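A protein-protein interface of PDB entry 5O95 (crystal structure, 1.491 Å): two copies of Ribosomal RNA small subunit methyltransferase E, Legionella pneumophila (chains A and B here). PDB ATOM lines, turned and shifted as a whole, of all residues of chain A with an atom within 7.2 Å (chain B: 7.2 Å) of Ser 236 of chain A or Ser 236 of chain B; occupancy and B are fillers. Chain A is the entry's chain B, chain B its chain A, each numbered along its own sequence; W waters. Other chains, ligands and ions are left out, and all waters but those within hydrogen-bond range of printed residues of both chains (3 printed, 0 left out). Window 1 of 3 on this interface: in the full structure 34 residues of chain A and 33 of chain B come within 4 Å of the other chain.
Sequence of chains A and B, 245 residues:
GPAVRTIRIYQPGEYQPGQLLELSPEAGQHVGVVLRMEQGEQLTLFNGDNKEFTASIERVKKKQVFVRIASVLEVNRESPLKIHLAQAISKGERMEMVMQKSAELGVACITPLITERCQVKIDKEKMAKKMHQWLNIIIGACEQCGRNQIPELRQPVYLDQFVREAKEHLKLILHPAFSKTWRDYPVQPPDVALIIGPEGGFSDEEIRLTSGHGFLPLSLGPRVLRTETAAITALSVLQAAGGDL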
ATOM      1  N   ILE A  83      36.301   7.777  19.244  1.00  0.00           N
ATOM      2  CA  ILE A  83      35.549   8.997  19.524  1.00  0.00           C
ATOM      3  C   ILE A  83      36.474   9.953  20.256  1.00  0.00           C
ATOM      4  O   ILE A  83      37.116   9.570  21.241  1.00  0.00           O
ATOM      5  CB  ILE A  83      34.317   8.697  20.384  1.00  0.00           C
ATOM      6  CG1 ILE A  83      33.456   7.610  19.718  1.00  0.00           C
ATOM      7  CG2 ILE A  83      33.530   9.981  20.626  1.00  0.00           C
ATOM      8  CD1 ILE A  83      32.268   7.186  20.570  1.00  0.00           C
ATOM      9  N   LEU A 105      33.023   3.958  28.507  1.00  0.00           N
ATOM     10  CA  LEU A 105      32.365   3.876  27.211  1.00  0.00           C
ATOM     11  C   LEU A 105      33.345   3.837  26.057  1.00  0.00           C
ATOM     12  O   LEU A 105      32.926   3.967  24.905  1.00  0.00           O
ATOM     13  CB  LEU A 105      31.347   5.027  27.038  1.00  0.00           C
ATOM     14  CG  LEU A 105      29.915   4.696  27.426  1.00  0.00           C
ATOM     15  CD1 LEU A 105      29.381   3.574  26.513  1.00  0.00           C
ATOM     16  CD2 LEU A 105      29.836   4.242  28.856  1.00  0.00           C
ATOM     17  N   TRP A 182      21.024  10.408  15.224  1.00  0.00           N
ATOM     18  CA  TRP A 182      22.118   9.501  14.886  1.00  0.00           C
ATOM     19  C   TRP A 182      21.849   8.750  13.585  1.00  0.00           C
ATOM     20  O   TRP A 182      22.794   8.341  12.898  1.00  0.00           O
ATOM     21  CB  TRP A 182      22.335   8.516  16.041  1.00  0.00           C
ATOM     22  CG  TRP A 182      21.180   7.549  16.232  1.00  0.00           C
ATOM     23  CD1 TRP A 182      20.097   7.707  17.057  1.00  0.00           C
ATOM     24  CD2 TRP A 182      21.011   6.279  15.592  1.00  0.00           C
ATOM     25  NE1 TRP A 182      19.260   6.619  16.951  1.00  0.00           N
ATOM     26  CE2 TRP A 182      19.797   5.731  16.060  1.00  0.00           C
ATOM     27  CE3 TRP A 182      21.767   5.553  14.666  1.00  0.00           C
ATOM     28  CZ2 TRP A 182      19.325   4.490  15.634  1.00  0.00           C
ATOM     29  CZ3 TRP A 182      21.291   4.319  14.238  1.00  0.00           C
ATOM     30  CH2 TRP A 182      20.081   3.803  14.725  1.00  0.00           C
ATOM     31  N   LEU A 220      19.589  14.459  20.815  1.00  0.00           N
ATOM     32  CA  LEU A 220      19.495  13.274  21.658  1.00  0.00           C
ATOM     33  C   LEU A 220      18.174  13.303  22.437  1.00  0.00           C
ATOM     34  O   LEU A 220      18.149  13.229  23.663  1.00  0.00           O
ATOM     35  CB  LEU A 220      20.691  13.128  22.599  1.00  0.00           C
ATOM     36  CG  LEU A 220      22.027  12.755  21.943  1.00  0.00           C
ATOM     37  CD1 LEU A 220      23.163  12.851  22.962  1.00  0.00           C
ATOM     38  CD2 LEU A 220      22.009  11.362  21.292  1.00  0.00           C
ATOM     39  N   LEU A 225      19.078  17.192  28.634  1.00  0.00           N
ATOM     40  CA  LEU A 225      19.969  16.380  29.432  1.00  0.00           C
ATOM     41  C   LEU A 225      20.969  17.264  30.153  1.00  0.00           C
ATOM     42  O   LEU A 225      21.454  18.249  29.599  1.00  0.00           O
ATOM     43  CB  LEU A 225      20.717  15.415  28.517  1.00  0.00           C
ATOM     44  CG  LEU A 225      19.846  14.462  27.688  1.00  0.00           C
ATOM     45  CD1 LEU A 225      20.750  13.588  26.840  1.00  0.00           C
ATOM     46  CD2 LEU A 225      18.959  13.601  28.572  1.00  0.00           C
ATOM     47  N   THR A 229      25.162  13.864  31.701  1.00  0.00           N
ATOM     48  CA  THR A 229      24.332  12.821  31.112  1.00  0.00           C
ATOM     49  C   THR A 229      24.494  12.811  29.606  1.00  0.00           C
ATOM     50  O   THR A 229      24.576  11.742  28.990  1.00  0.00           O
ATOM     51  CB  THR A 229      22.872  13.102  31.453  1.00  0.00           C
ATOM     52  OG1 THR A 229      22.729  13.260  32.862  1.00  0.00           O
ATOM     53  CG2 THR A 229      21.996  11.916  30.999  1.00  0.00           C
ATOM     54  N   ALA A 230      24.517  13.993  28.997  1.00  0.00           N
ATOM     55  CA  ALA A 230      24.624  14.114  27.554  1.00  0.00           C
ATOM     56  C   ALA A 230      25.887  13.451  27.034  1.00  0.00           C
ATOM     57  O   ALA A 230      25.850  12.780  26.004  1.00  0.00           O
ATOM     58  CB  ALA A 230      24.609  15.585  27.139  1.00  0.00           C
ATOM     59  N   ALA A 231      27.024  13.696  27.689  1.00  0.00           N
ATOM     60  CA  ALA A 231      28.259  13.038  27.279  1.00  0.00           C
ATOM     61  C   ALA A 231      28.095  11.533  27.245  1.00  0.00           C
ATOM     62  O   ALA A 231      28.469  10.880  26.266  1.00  0.00           O
ATOM     63  CB  ALA A 231      29.393  13.415  28.231  1.00  0.00           C
ATOM     64  N   ILE A 232      27.571  10.958  28.323  1.00  0.00           N
ATOM     65  CA  ILE A 232      27.550   9.499  28.384  1.00  0.00           C
ATOM     66  C   ILE A 232      26.465   8.933  27.467  1.00  0.00           C
ATOM     67  O   ILE A 232      26.643   7.874  26.866  1.00  0.00           O
ATOM     68  CB  ILE A 232      27.471   9.017  29.842  1.00  0.00           C
ATOM     69  CG1 ILE A 232      28.582   9.684  30.675  1.00  0.00           C
ATOM     70  CG2 ILE A 232      27.672   7.494  29.915  1.00  0.00           C
ATOM     71  CD1 ILE A 232      29.976   9.796  29.965  1.00  0.00           C
ATOM     72  N   THR A 233      25.340   9.634  27.312  1.00  0.00           N
ATOM     73  CA  THR A 233      24.324   9.214  26.355  1.00  0.00           C
ATOM     74  C   THR A 233      24.844   9.269  24.921  1.00  0.00           C
ATOM     75  O   THR A 233      24.606   8.347  24.125  1.00  0.00           O
ATOM     76  CB  THR A 233      23.097  10.145  26.513  1.00  0.00           C
ATOM     77  OG1 THR A 233      22.544   9.946  27.828  1.00  0.00           O
ATOM     78  CG2 THR A 233      22.041   9.880  25.443  1.00  0.00           C
ATOM     79  N   ALA A 234      25.559  10.335  24.565  1.00  0.00           N
ATOM     80  CA  ALA A 234      26.072  10.452  23.206  1.00  0.00           C
ATOM     81  C   ALA A 234      27.094   9.356  22.917  1.00  0.00           C
ATOM     82  O   ALA A 234      27.061   8.726  21.855  1.00  0.00           O
ATOM     83  CB  ALA A 234      26.721  11.829  23.014  1.00  0.00           C
ATOM     84  N   LEU A 235      28.019   9.133  23.849  1.00  0.00           N
ATOM     85  CA  LEU A 235      29.006   8.076  23.650  1.00  0.00           C
ATOM     86  C   LEU A 235      28.342   6.716  23.510  1.00  0.00           C
ATOM     87  O   LEU A 235      28.758   5.899  22.678  1.00  0.00           O
ATOM     88  CB  LEU A 235      30.007   8.052  24.795  1.00  0.00           C
ATOM     89  CG  LEU A 235      30.932   9.266  24.859  1.00  0.00           C
ATOM     90  CD1 LEU A 235      31.864   9.134  26.005  1.00  0.00           C
ATOM     91  CD2 LEU A 235      31.694   9.411  23.562  1.00  0.00           C
ATOM     92  N   SER A 236      27.305   6.453  24.312  1.00  0.00           N
ATOM     93  CA  SER A 236      26.601   5.169  24.209  1.00  0.00           C
ATOM     94  C   SER A 236      25.948   5.016  22.844  1.00  0.00           C
ATOM     95  O   SER A 236      26.006   3.948  22.224  1.00  0.00           O
ATOM     96  CB  SER A 236      25.525   5.087  25.300  1.00  0.00           C
ATOM     97  OG  SER A 236      26.039   5.162  26.616  1.00  0.00           O
ATOM     98  N   VAL A 237      25.271   6.070  22.382  1.00  0.00           N
ATOM     99  CA  VAL A 237      24.572   5.982  21.110  1.00  0.00           C
ATOM    100  C   VAL A 237      25.565   5.845  19.965  1.00  0.00           C
ATOM    101  O   VAL A 237      25.370   5.037  19.054  1.00  0.00           O
ATOM    102  CB  VAL A 237      23.639   7.192  20.923  1.00  0.00           C
ATOM    103  CG1 VAL A 237      23.065   7.195  19.516  1.00  0.00           C
ATOM    104  CG2 VAL A 237      22.528   7.185  21.967  1.00  0.00           C
ATOM    105  N   LEU A 238      26.671   6.600  20.016  1.00  0.00           N
ATOM    106  CA  LEU A 238      27.667   6.516  18.951  1.00  0.00           C
ATOM    107  C   LEU A 238      28.377   5.165  18.949  1.00  0.00           C
ATOM    108  O   LEU A 238      28.602   4.592  17.884  1.00  0.00           O
ATOM    109  CB  LEU A 238      28.689   7.648  19.100  1.00  0.00           C
ATOM    110  CG  LEU A 238      28.094   9.043  18.904  1.00  0.00           C
ATOM    111  CD1 LEU A 238      29.158  10.095  19.227  1.00  0.00           C
ATOM    112  CD2 LEU A 238      27.567   9.213  17.485  1.00  0.00           C
ATOM    113  N   GLN A 239      28.702   4.628  20.129  1.00  0.00           N
ATOM    114  CA  GLN A 239      29.343   3.315  20.171  1.00  0.00           C
ATOM    115  C   GLN A 239      28.398   2.218  19.728  1.00  0.00           C
ATOM    116  O   GLN A 239      28.832   1.216  19.159  1.00  0.00           O
ATOM    117  CB  GLN A 239      29.842   2.998  21.572  1.00  0.00           C
ATOM    118  CG  GLN A 239      31.042   3.825  22.013  1.00  0.00           C
ATOM    119  CD  GLN A 239      32.353   3.445  21.304  1.00  0.00           C
ATOM    120  OE1 GLN A 239      32.372   2.765  20.273  1.00  0.00           O
ATOM    121  NE2 GLN A 239      33.454   3.918  21.872  1.00  0.00           N
ATOM    122  N   ALA A 240      27.106   2.361  20.005  1.00  0.00           N
ATOM    123  CA  ALA A 240      26.177   1.346  19.516  1.00  0.00           C
ATOM    124  C   ALA A 240      26.023   1.434  18.002  1.00  0.00           C
ATOM    125  O   ALA A 240      26.025   0.409  17.309  1.00  0.00           O
ATOM    126  CB  ALA A 240      24.829   1.520  20.225  1.00  0.00           C
ATOM    127  N   ALA A 241      25.929   2.655  17.469  1.00  0.00           N
ATOM    128  CA  ALA A 241      25.700   2.837  16.041  1.00  0.00           C
ATOM    129  C   ALA A 241      26.922   2.446  15.215  1.00  0.00           C
ATOM    130  O   ALA A 241      26.783   1.797  14.173  1.00  0.00           O
ATOM    131  CB  ALA A 241      25.294   4.287  15.756  1.00  0.00           C
ATOM    132  N   GLY A 242      28.127   2.802  15.673  1.00  0.00           N
ATOM    133  CA  GLY A 242      29.304   2.606  14.842  1.00  0.00           C
ATOM    134  C   GLY A 242      30.474   1.915  15.508  1.00  0.00           C
ATOM    135  O   GLY A 242      31.506   1.693  14.868  1.00  0.00           O
ATOM    136  N   LEU A 245      29.287  -1.551  20.845  1.00  0.00           N
ATOM    137  CA  LEU A 245      28.146  -1.897  21.678  1.00  0.00           C
ATOM    138  C   LEU A 245      27.090  -2.594  20.839  1.00  0.00           C
ATOM    139  O   LEU A 245      26.844  -2.191  19.702  1.00  0.00           O
ATOM    140  CB  LEU A 245      27.545  -0.658  22.323  1.00  0.00           C
ATOM    141  CG  LEU A 245      28.053  -0.350  23.724  1.00  0.00           C
ATOM    142  CD1 LEU A 245      29.549  -0.231  23.761  1.00  0.00           C
ATOM    143  CD2 LEU A 245      27.412   0.940  24.198  1.00  0.00           C
ATOM    144  OXT LEU A 245      26.469  -3.564  21.277  1.00  0.00           O
ATOM    145  N   ILE B  83       9.962   2.205  28.928  1.00  0.00           N
ATOM    146  CA  ILE B  83      10.926   1.276  29.497  1.00  0.00           C
ATOM    147  C   ILE B  83      10.613   1.133  30.974  1.00  0.00           C
ATOM    148  O   ILE B  83      10.500   2.139  31.692  1.00  0.00           O
ATOM    149  CB  ILE B  83      12.373   1.763  29.293  1.00  0.00           C
ATOM    150  CG1 ILE B  83      12.631   2.043  27.805  1.00  0.00           C
ATOM    151  CG2 ILE B  83      13.349   0.775  29.929  1.00  0.00           C
ATOM    152  CD1 ILE B  83      14.100   2.382  27.447  1.00  0.00           C
ATOM    153  N   LEU B 105      16.494  10.188  30.924  1.00  0.00           N
ATOM    154  CA  LEU B 105      16.474   9.371  29.724  1.00  0.00           C
ATOM    155  C   LEU B 105      15.095   8.778  29.446  1.00  0.00           C
ATOM    156  O   LEU B 105      14.960   7.865  28.612  1.00  0.00           O
ATOM    157  CB  LEU B 105      17.572   8.287  29.827  1.00  0.00           C
ATOM    158  CG  LEU B 105      18.980   8.887  29.832  1.00  0.00           C
ATOM    159  CD1 LEU B 105      20.035   7.845  30.216  1.00  0.00           C
ATOM    160  CD2 LEU B 105      19.319   9.471  28.481  1.00  0.00           C
ATOM    161  N   TRP B 182      21.934  -5.108  20.513  1.00  0.00           N
ATOM    162  CA  TRP B 182      20.726  -4.451  20.014  1.00  0.00           C
ATOM    163  C   TRP B 182      20.369  -4.910  18.603  1.00  0.00           C
ATOM    164  O   TRP B 182      19.193  -4.859  18.219  1.00  0.00           O
ATOM    165  CB  TRP B 182      20.861  -2.922  20.083  1.00  0.00           C
ATOM    166  CG  TRP B 182      21.963  -2.361  19.231  1.00  0.00           C
ATOM    167  CD1 TRP B 182      23.251  -2.126  19.617  1.00  0.00           C
ATOM    168  CD2 TRP B 182      21.887  -1.988  17.845  1.00  0.00           C
ATOM    169  NE1 TRP B 182      23.982  -1.633  18.560  1.00  0.00           N
ATOM    170  CE2 TRP B 182      23.169  -1.546  17.459  1.00  0.00           C
ATOM    171  CE3 TRP B 182      20.863  -2.003  16.891  1.00  0.00           C
ATOM    172  CZ2 TRP B 182      23.449  -1.101  16.167  1.00  0.00           C
ATOM    173  CZ3 TRP B 182      21.147  -1.574  15.608  1.00  0.00           C
ATOM    174  CH2 TRP B 182      22.425  -1.123  15.259  1.00  0.00           C
ATOM    175  N   LEU B 220      26.406  -5.072  26.127  1.00  0.00           N
ATOM    176  CA  LEU B 220      26.675  -3.681  25.806  1.00  0.00           C
ATOM    177  C   LEU B 220      28.180  -3.473  25.785  1.00  0.00           C
ATOM    178  O   LEU B 220      28.732  -2.711  26.570  1.00  0.00           O
ATOM    179  CB  LEU B 220      26.085  -2.740  26.852  1.00  0.00           C
ATOM    180  CG  LEU B 220      24.545  -2.692  26.903  1.00  0.00           C
ATOM    181  CD1 LEU B 220      24.082  -1.964  28.148  1.00  0.00           C
ATOM    182  CD2 LEU B 220      24.022  -2.049  25.629  1.00  0.00           C
ATOM    183  N   LEU B 225      30.963  -2.315  32.668  1.00  0.00           N
ATOM    184  CA  LEU B 225      30.355  -1.041  33.034  1.00  0.00           C
ATOM    185  C   LEU B 225      29.976  -1.070  34.506  1.00  0.00           C
ATOM    186  O   LEU B 225      29.441  -2.065  34.998  1.00  0.00           O
ATOM    187  CB  LEU B 225      29.105  -0.803  32.191  1.00  0.00           C
ATOM    188  CG  LEU B 225      29.319  -0.705  30.675  1.00  0.00           C
ATOM    189  CD1 LEU B 225      28.013  -0.413  29.907  1.00  0.00           C
ATOM    190  CD2 LEU B 225      30.450   0.322  30.369  1.00  0.00           C
ATOM    191  N   THR B 229      26.587   3.265  35.267  1.00  0.00           N
ATOM    192  CA  THR B 229      26.855   3.503  33.860  1.00  0.00           C
ATOM    193  C   THR B 229      26.007   2.586  32.982  1.00  0.00           C
ATOM    194  O   THR B 229      25.536   2.997  31.916  1.00  0.00           O
ATOM    195  CB  THR B 229      28.334   3.229  33.594  1.00  0.00           C
ATOM    196  OG1 THR B 229      29.116   3.936  34.550  1.00  0.00           O
ATOM    197  CG2 THR B 229      28.728   3.661  32.161  1.00  0.00           C
ATOM    198  N   ALA B 230      25.847   1.319  33.383  1.00  0.00           N
ATOM    199  CA  ALA B 230      25.073   0.377  32.575  1.00  0.00           C
ATOM    200  C   ALA B 230      23.639   0.847  32.399  1.00  0.00           C
ATOM    201  O   ALA B 230      23.051   0.685  31.323  1.00  0.00           O
ATOM    202  CB  ALA B 230      25.102  -1.006  33.219  1.00  0.00           C
ATOM    203  N   ALA B 231      23.082   1.464  33.441  1.00  0.00           N
ATOM    204  CA  ALA B 231      21.719   1.981  33.362  1.00  0.00           C
ATOM    205  C   ALA B 231      21.622   3.106  32.345  1.00  0.00           C
ATOM    206  O   ALA B 231      20.735   3.100  31.483  1.00  0.00           O
ATOM    207  CB  ALA B 231      21.260   2.451  34.743  1.00  0.00           C
ATOM    208  N   ILE B 232      22.537   4.073  32.421  1.00  0.00           N
ATOM    209  CA  ILE B 232      22.575   5.171  31.451  1.00  0.00           C
ATOM    210  C   ILE B 232      22.747   4.626  30.046  1.00  0.00           C
ATOM    211  O   ILE B 232      22.051   5.026  29.104  1.00  0.00           O
ATOM    212  CB  ILE B 232      23.743   6.128  31.766  1.00  0.00           C
ATOM    213  CG1 ILE B 232      23.673   6.703  33.172  1.00  0.00           C
ATOM    214  CG2 ILE B 232      23.839   7.221  30.699  1.00  0.00           C
ATOM    215  CD1 ILE B 232      24.923   7.520  33.491  1.00  0.00           C
ATOM    216  N   THR B 233      23.726   3.733  29.869  1.00  0.00           N
ATOM    217  CA  THR B 233      24.044   3.252  28.536  1.00  0.00           C
ATOM    218  C   THR B 233      22.903   2.426  27.963  1.00  0.00           C
ATOM    219  O   THR B 233      22.537   2.593  26.795  1.00  0.00           O
ATOM    220  CB  THR B 233      25.338   2.422  28.607  1.00  0.00           C
ATOM    221  OG1 THR B 233      26.397   3.302  28.996  1.00  0.00           O
ATOM    222  CG2 THR B 233      25.679   1.808  27.275  1.00  0.00           C
ATOM    223  N   ALA B 234      22.328   1.544  28.774  1.00  0.00           N
ATOM    224  CA  ALA B 234      21.240   0.700  28.279  1.00  0.00           C
ATOM    225  C   ALA B 234      20.017   1.539  27.899  1.00  0.00           C
ATOM    226  O   ALA B 234      19.413   1.315  26.845  1.00  0.00           O
ATOM    227  CB  ALA B 234      20.854  -0.350  29.325  1.00  0.00           C
ATOM    228  N   LEU B 235      19.651   2.517  28.731  1.00  0.00           N
ATOM    229  CA  LEU B 235      18.495   3.339  28.388  1.00  0.00           C
ATOM    230  C   LEU B 235      18.777   4.186  27.150  1.00  0.00           C
ATOM    231  O   LEU B 235      17.907   4.340  26.292  1.00  0.00           O
ATOM    232  CB  LEU B 235      18.095   4.212  29.574  1.00  0.00           C
ATOM    233  CG  LEU B 235      17.583   3.477  30.807  1.00  0.00           C
ATOM    234  CD1 LEU B 235      17.353   4.455  31.934  1.00  0.00           C
ATOM    235  CD2 LEU B 235      16.289   2.771  30.481  1.00  0.00           C
ATOM    236  N   SER B 236      20.008   4.714  27.025  1.00  0.00           N
ATOM    237  CA  SER B 236      20.362   5.468  25.823  1.00  0.00           C
ATOM    238  C   SER B 236      20.237   4.616  24.578  1.00  0.00           C
ATOM    239  O   SER B 236      19.696   5.057  23.559  1.00  0.00           O
ATOM    240  CB  SER B 236      21.787   6.012  25.930  1.00  0.00           C
ATOM    241  OG  SER B 236      21.920   6.847  27.048  1.00  0.00           O
ATOM    242  N   VAL B 237      20.791   3.397  24.625  1.00  0.00           N
ATOM    243  CA  VAL B 237      20.779   2.512  23.467  1.00  0.00           C
ATOM    244  C   VAL B 237      19.349   2.129  23.111  1.00  0.00           C
ATOM    245  O   VAL B 237      18.948   2.223  21.953  1.00  0.00           O
ATOM    246  CB  VAL B 237      21.690   1.295  23.711  1.00  0.00           C
ATOM    247  CG1 VAL B 237      21.469   0.239  22.637  1.00  0.00           C
ATOM    248  CG2 VAL B 237      23.140   1.732  23.728  1.00  0.00           C
ATOM    249  N   LEU B 238      18.557   1.740  24.113  1.00  0.00           N
ATOM    250  CA  LEU B 238      17.163   1.379  23.859  1.00  0.00           C
ATOM    251  C   LEU B 238      16.360   2.555  23.292  1.00  0.00           C
ATOM    252  O   LEU B 238      15.630   2.395  22.303  1.00  0.00           O
ATOM    253  CB  LEU B 238      16.520   0.804  25.127  1.00  0.00           C
ATOM    254  CG  LEU B 238      17.164  -0.551  25.496  1.00  0.00           C
ATOM    255  CD1 LEU B 238      16.676  -0.995  26.868  1.00  0.00           C
ATOM    256  CD2 LEU B 238      16.898  -1.655  24.463  1.00  0.00           C
ATOM    257  N   GLN B 239      16.498   3.755  23.880  1.00  0.00           N
ATOM    258  CA  GLN B 239      15.750   4.901  23.352  1.00  0.00           C
ATOM    259  C   GLN B 239      16.224   5.290  21.959  1.00  0.00           C
ATOM    260  O   GLN B 239      15.433   5.761  21.140  1.00  0.00           O
ATOM    261  CB  GLN B 239      15.866   6.115  24.275  1.00  0.00           C
ATOM    262  CG  GLN B 239      15.331   5.921  25.674  1.00  0.00           C
ATOM    263  CD  GLN B 239      13.836   5.979  25.733  1.00  0.00           C
ATOM    264  OE1 GLN B 239      13.172   5.788  24.726  1.00  0.00           O
ATOM    265  NE2 GLN B 239      13.297   6.253  26.915  1.00  0.00           N
ATOM    266  N   ALA B 240      17.522   5.160  21.678  1.00  0.00           N
ATOM    267  CA  ALA B 240      17.978   5.450  20.320  1.00  0.00           C
ATOM    268  C   ALA B 240      17.459   4.403  19.334  1.00  0.00           C
ATOM    269  O   ALA B 240      17.168   4.723  18.178  1.00  0.00           O
ATOM    270  CB  ALA B 240      19.513   5.473  20.272  1.00  0.00           C
ATOM    271  N   ALA B 241      17.388   3.141  19.760  1.00  0.00           N
ATOM    272  CA  ALA B 241      16.975   2.061  18.862  1.00  0.00           C
ATOM    273  C   ALA B 241      15.475   2.106  18.578  1.00  0.00           C
ATOM    274  O   ALA B 241      15.050   1.924  17.431  1.00  0.00           O
ATOM    275  CB  ALA B 241      17.348   0.702  19.462  1.00  0.00           C
ATOM    276  N   GLY B 242      14.662   2.308  19.609  1.00  0.00           N
ATOM    277  CA  GLY B 242      13.225   2.179  19.450  1.00  0.00           C
ATOM    278  C   GLY B 242      12.412   3.285  20.071  1.00  0.00           C
ATOM    279  O   GLY B 242      11.180   3.237  20.038  1.00  0.00           O
ATOM    280  N   LEU B 245      15.326   8.982  20.831  1.00  0.00           N
ATOM    281  CA  LEU B 245      16.674   9.539  20.678  1.00  0.00           C
ATOM    282  C   LEU B 245      17.150   9.424  19.228  1.00  0.00           C
ATOM    283  O   LEU B 245      16.855   8.432  18.535  1.00  0.00           O
ATOM    284  CB  LEU B 245      17.681   8.864  21.627  1.00  0.00           C
ATOM    285  CG  LEU B 245      18.009   9.644  22.903  1.00  0.00           C
ATOM    286  CD1 LEU B 245      16.716   9.972  23.685  1.00  0.00           C
ATOM    287  CD2 LEU B 245      19.006   8.851  23.748  1.00  0.00           C
ATOM    288  OXT LEU B 245      17.832  10.324  18.718  1.00  0.00           O
HETATM  289  O   HOH W   1      16.576   8.478  15.889  1.00  0.00           O
HETATM  290  O   HOH W   2      24.022  -3.862  22.234  1.00  0.00           O
HETATM  291  O   HOH W   3      20.363  10.879  17.920  1.00  0.00           O
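Water W2 bridges the chain-end carboxylate of Leu 245 of chain A (2.6 Å) and the backbone NH of Trp 182 of chain B (3.0 Å).
Water W1 bridges the chain-end carboxylate (O) of Leu 245 of chain B (2.7 Å) and the indole nitrogen (NE1) of Trp 182 of chain A (3.4 Å).
Water W3 lies within hydrogen-bond range of OXT of Leu 245 of chain B and N of Trp 182 of chain A.
Leu 105 of chain A touches Thr 229 of chain B, but with the chains exchanged Thr 229 of chain A does not touch Leu 105 of chain B (4.4 Å).
Ile 232 of chain A touches its own counterpart, Ile 232 of chain B.
Ser 236 of chain B touches its own counterpart, Ser 236 of chain A.
Val 237 of chain A touches Ala 240 of chain B, and with the chains exchanged Ala 240 of chain A touches Val 237 of chain B.
The indole nitrogen (NE1) of Trp 182 of chain B is in hydrogen-bond range of the backbone carbonyl oxygen (O) of Ala 240 of chain A (3.1 Å).
NE1 of Trp 182 of chain B sits at hydrogen-bond distance from O of Leu 245 of chain A.
OG of Ser 236 of chain A sits at hydrogen-bond distance from OG1 of Thr 233 of chain B.
The side-chain hydroxyl (OG) of Ser 236 of chain B lies within hydrogen-bond range of the side-chain hydroxyl (OG1) of Thr 233 of chain A, at 3.3 Å.
The backbone carbonyl oxygen (O) of Ala 240 of chain B sits at hydrogen-bond distance from the indole nitrogen (NE1) of Trp 182 of chain A (3.1 Å).
NE1 of Trp 182 of chain A is in hydrogen-bond range of O of Leu 245 of chain B (3.4 Å).
Ser 236 of chain A touches just these residues of chain B: Thr 233, Ser 236 and Val 237.
Of the printed residues of chain A, Ser 236 of chain B touches Thr 233, Ser 236 and Val 237.
Of the printed residues of chain B, Val 237 of chain A touches Ser 236 (3.9 Å) and Ala 240 (3.9 Å).
Of the printed residues of chain B, Leu 220 of chain A touches Leu 245.
Printed residues of chain B within 4 Å of Leu 245 of chain A: Trp 182, Leu 220 and Thr 233.
Ala 230 of chain A touches none of the printed residues of chain B.
Ala 234 of chain A touches none of the printed residues of chain B.
O of Leu 105 of chain B sits at hydrogen-bond distance from NE2 of Gln 239 of chain B (2.9 Å).
The side-chain hydroxyl (OG) of Ser 236 of chain B lies within hydrogen-bond range of the backbone carbonyl oxygen (O) of Ile 232 of chain B.
The backbone carbonyl oxygen of Gln 239 of chain B sits at hydrogen-bond distance from the backbone NH of Leu 245 of chain B.
The backbone carbonyl oxygen (O) of Leu 105 of chain A is in hydrogen-bond range of the side-chain amide nitrogen (NE2) of Gln 239 of chain A (3.1 Å).
Thr 229 of chain B touches Leu 105 of chain A (CG2 to CD2, 3.5 Å).
CD2 of Leu 105 of chain A touches OG1 of Thr 233 of chain B, at 3.6 Å.
Leu 220 of chain A touches Leu 245 of chain B.
CG2 of Ile 232 of chain B touches CG2 of Ile 232 of chain A (3.9 Å).
CB of Ser 236 of chain B touches CB of Ser 236 of chain A, 3.9 Å away.
O of Ser 236 of chain B touches CG2 of Val 237 of chain A, 3.9 Å away.
CB of Ala 240 of chain B touches CG2 of Val 237 of chain A, 3.9 Å away.
Of the 20 printed residues of chain A, 9 touch a printed residue of chain B.
Printed residues of chain A that touch a printed residue of chain B: Leu 105, Trp 182, Leu 220, Ile 232, Thr 233, Ser 236, Val 237, Ala 240 and Leu 245.
Hydrophobic or aromatic side chains of chain A that line the printed part of chain B: Leu 105, Trp 182, Ile 232, Val 237, Ala 240 and Leu 245.
Of the 20 printed residues of chain B, 10 touch a printed residue of chain A.
Hydrophobic or aromatic side chains of chain B within 4 Å of the printed part of chain A: Leu 105, Trp 182, Ile 232, Val 237, Ala 240 and Leu 245.
Among the printed residues, 19 pairs touch across the chains.
Among the printed residues, no Asp or Glu carboxylate lies within 4 Å of a Lys or Arg side-chain nitrogen of the other chain.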
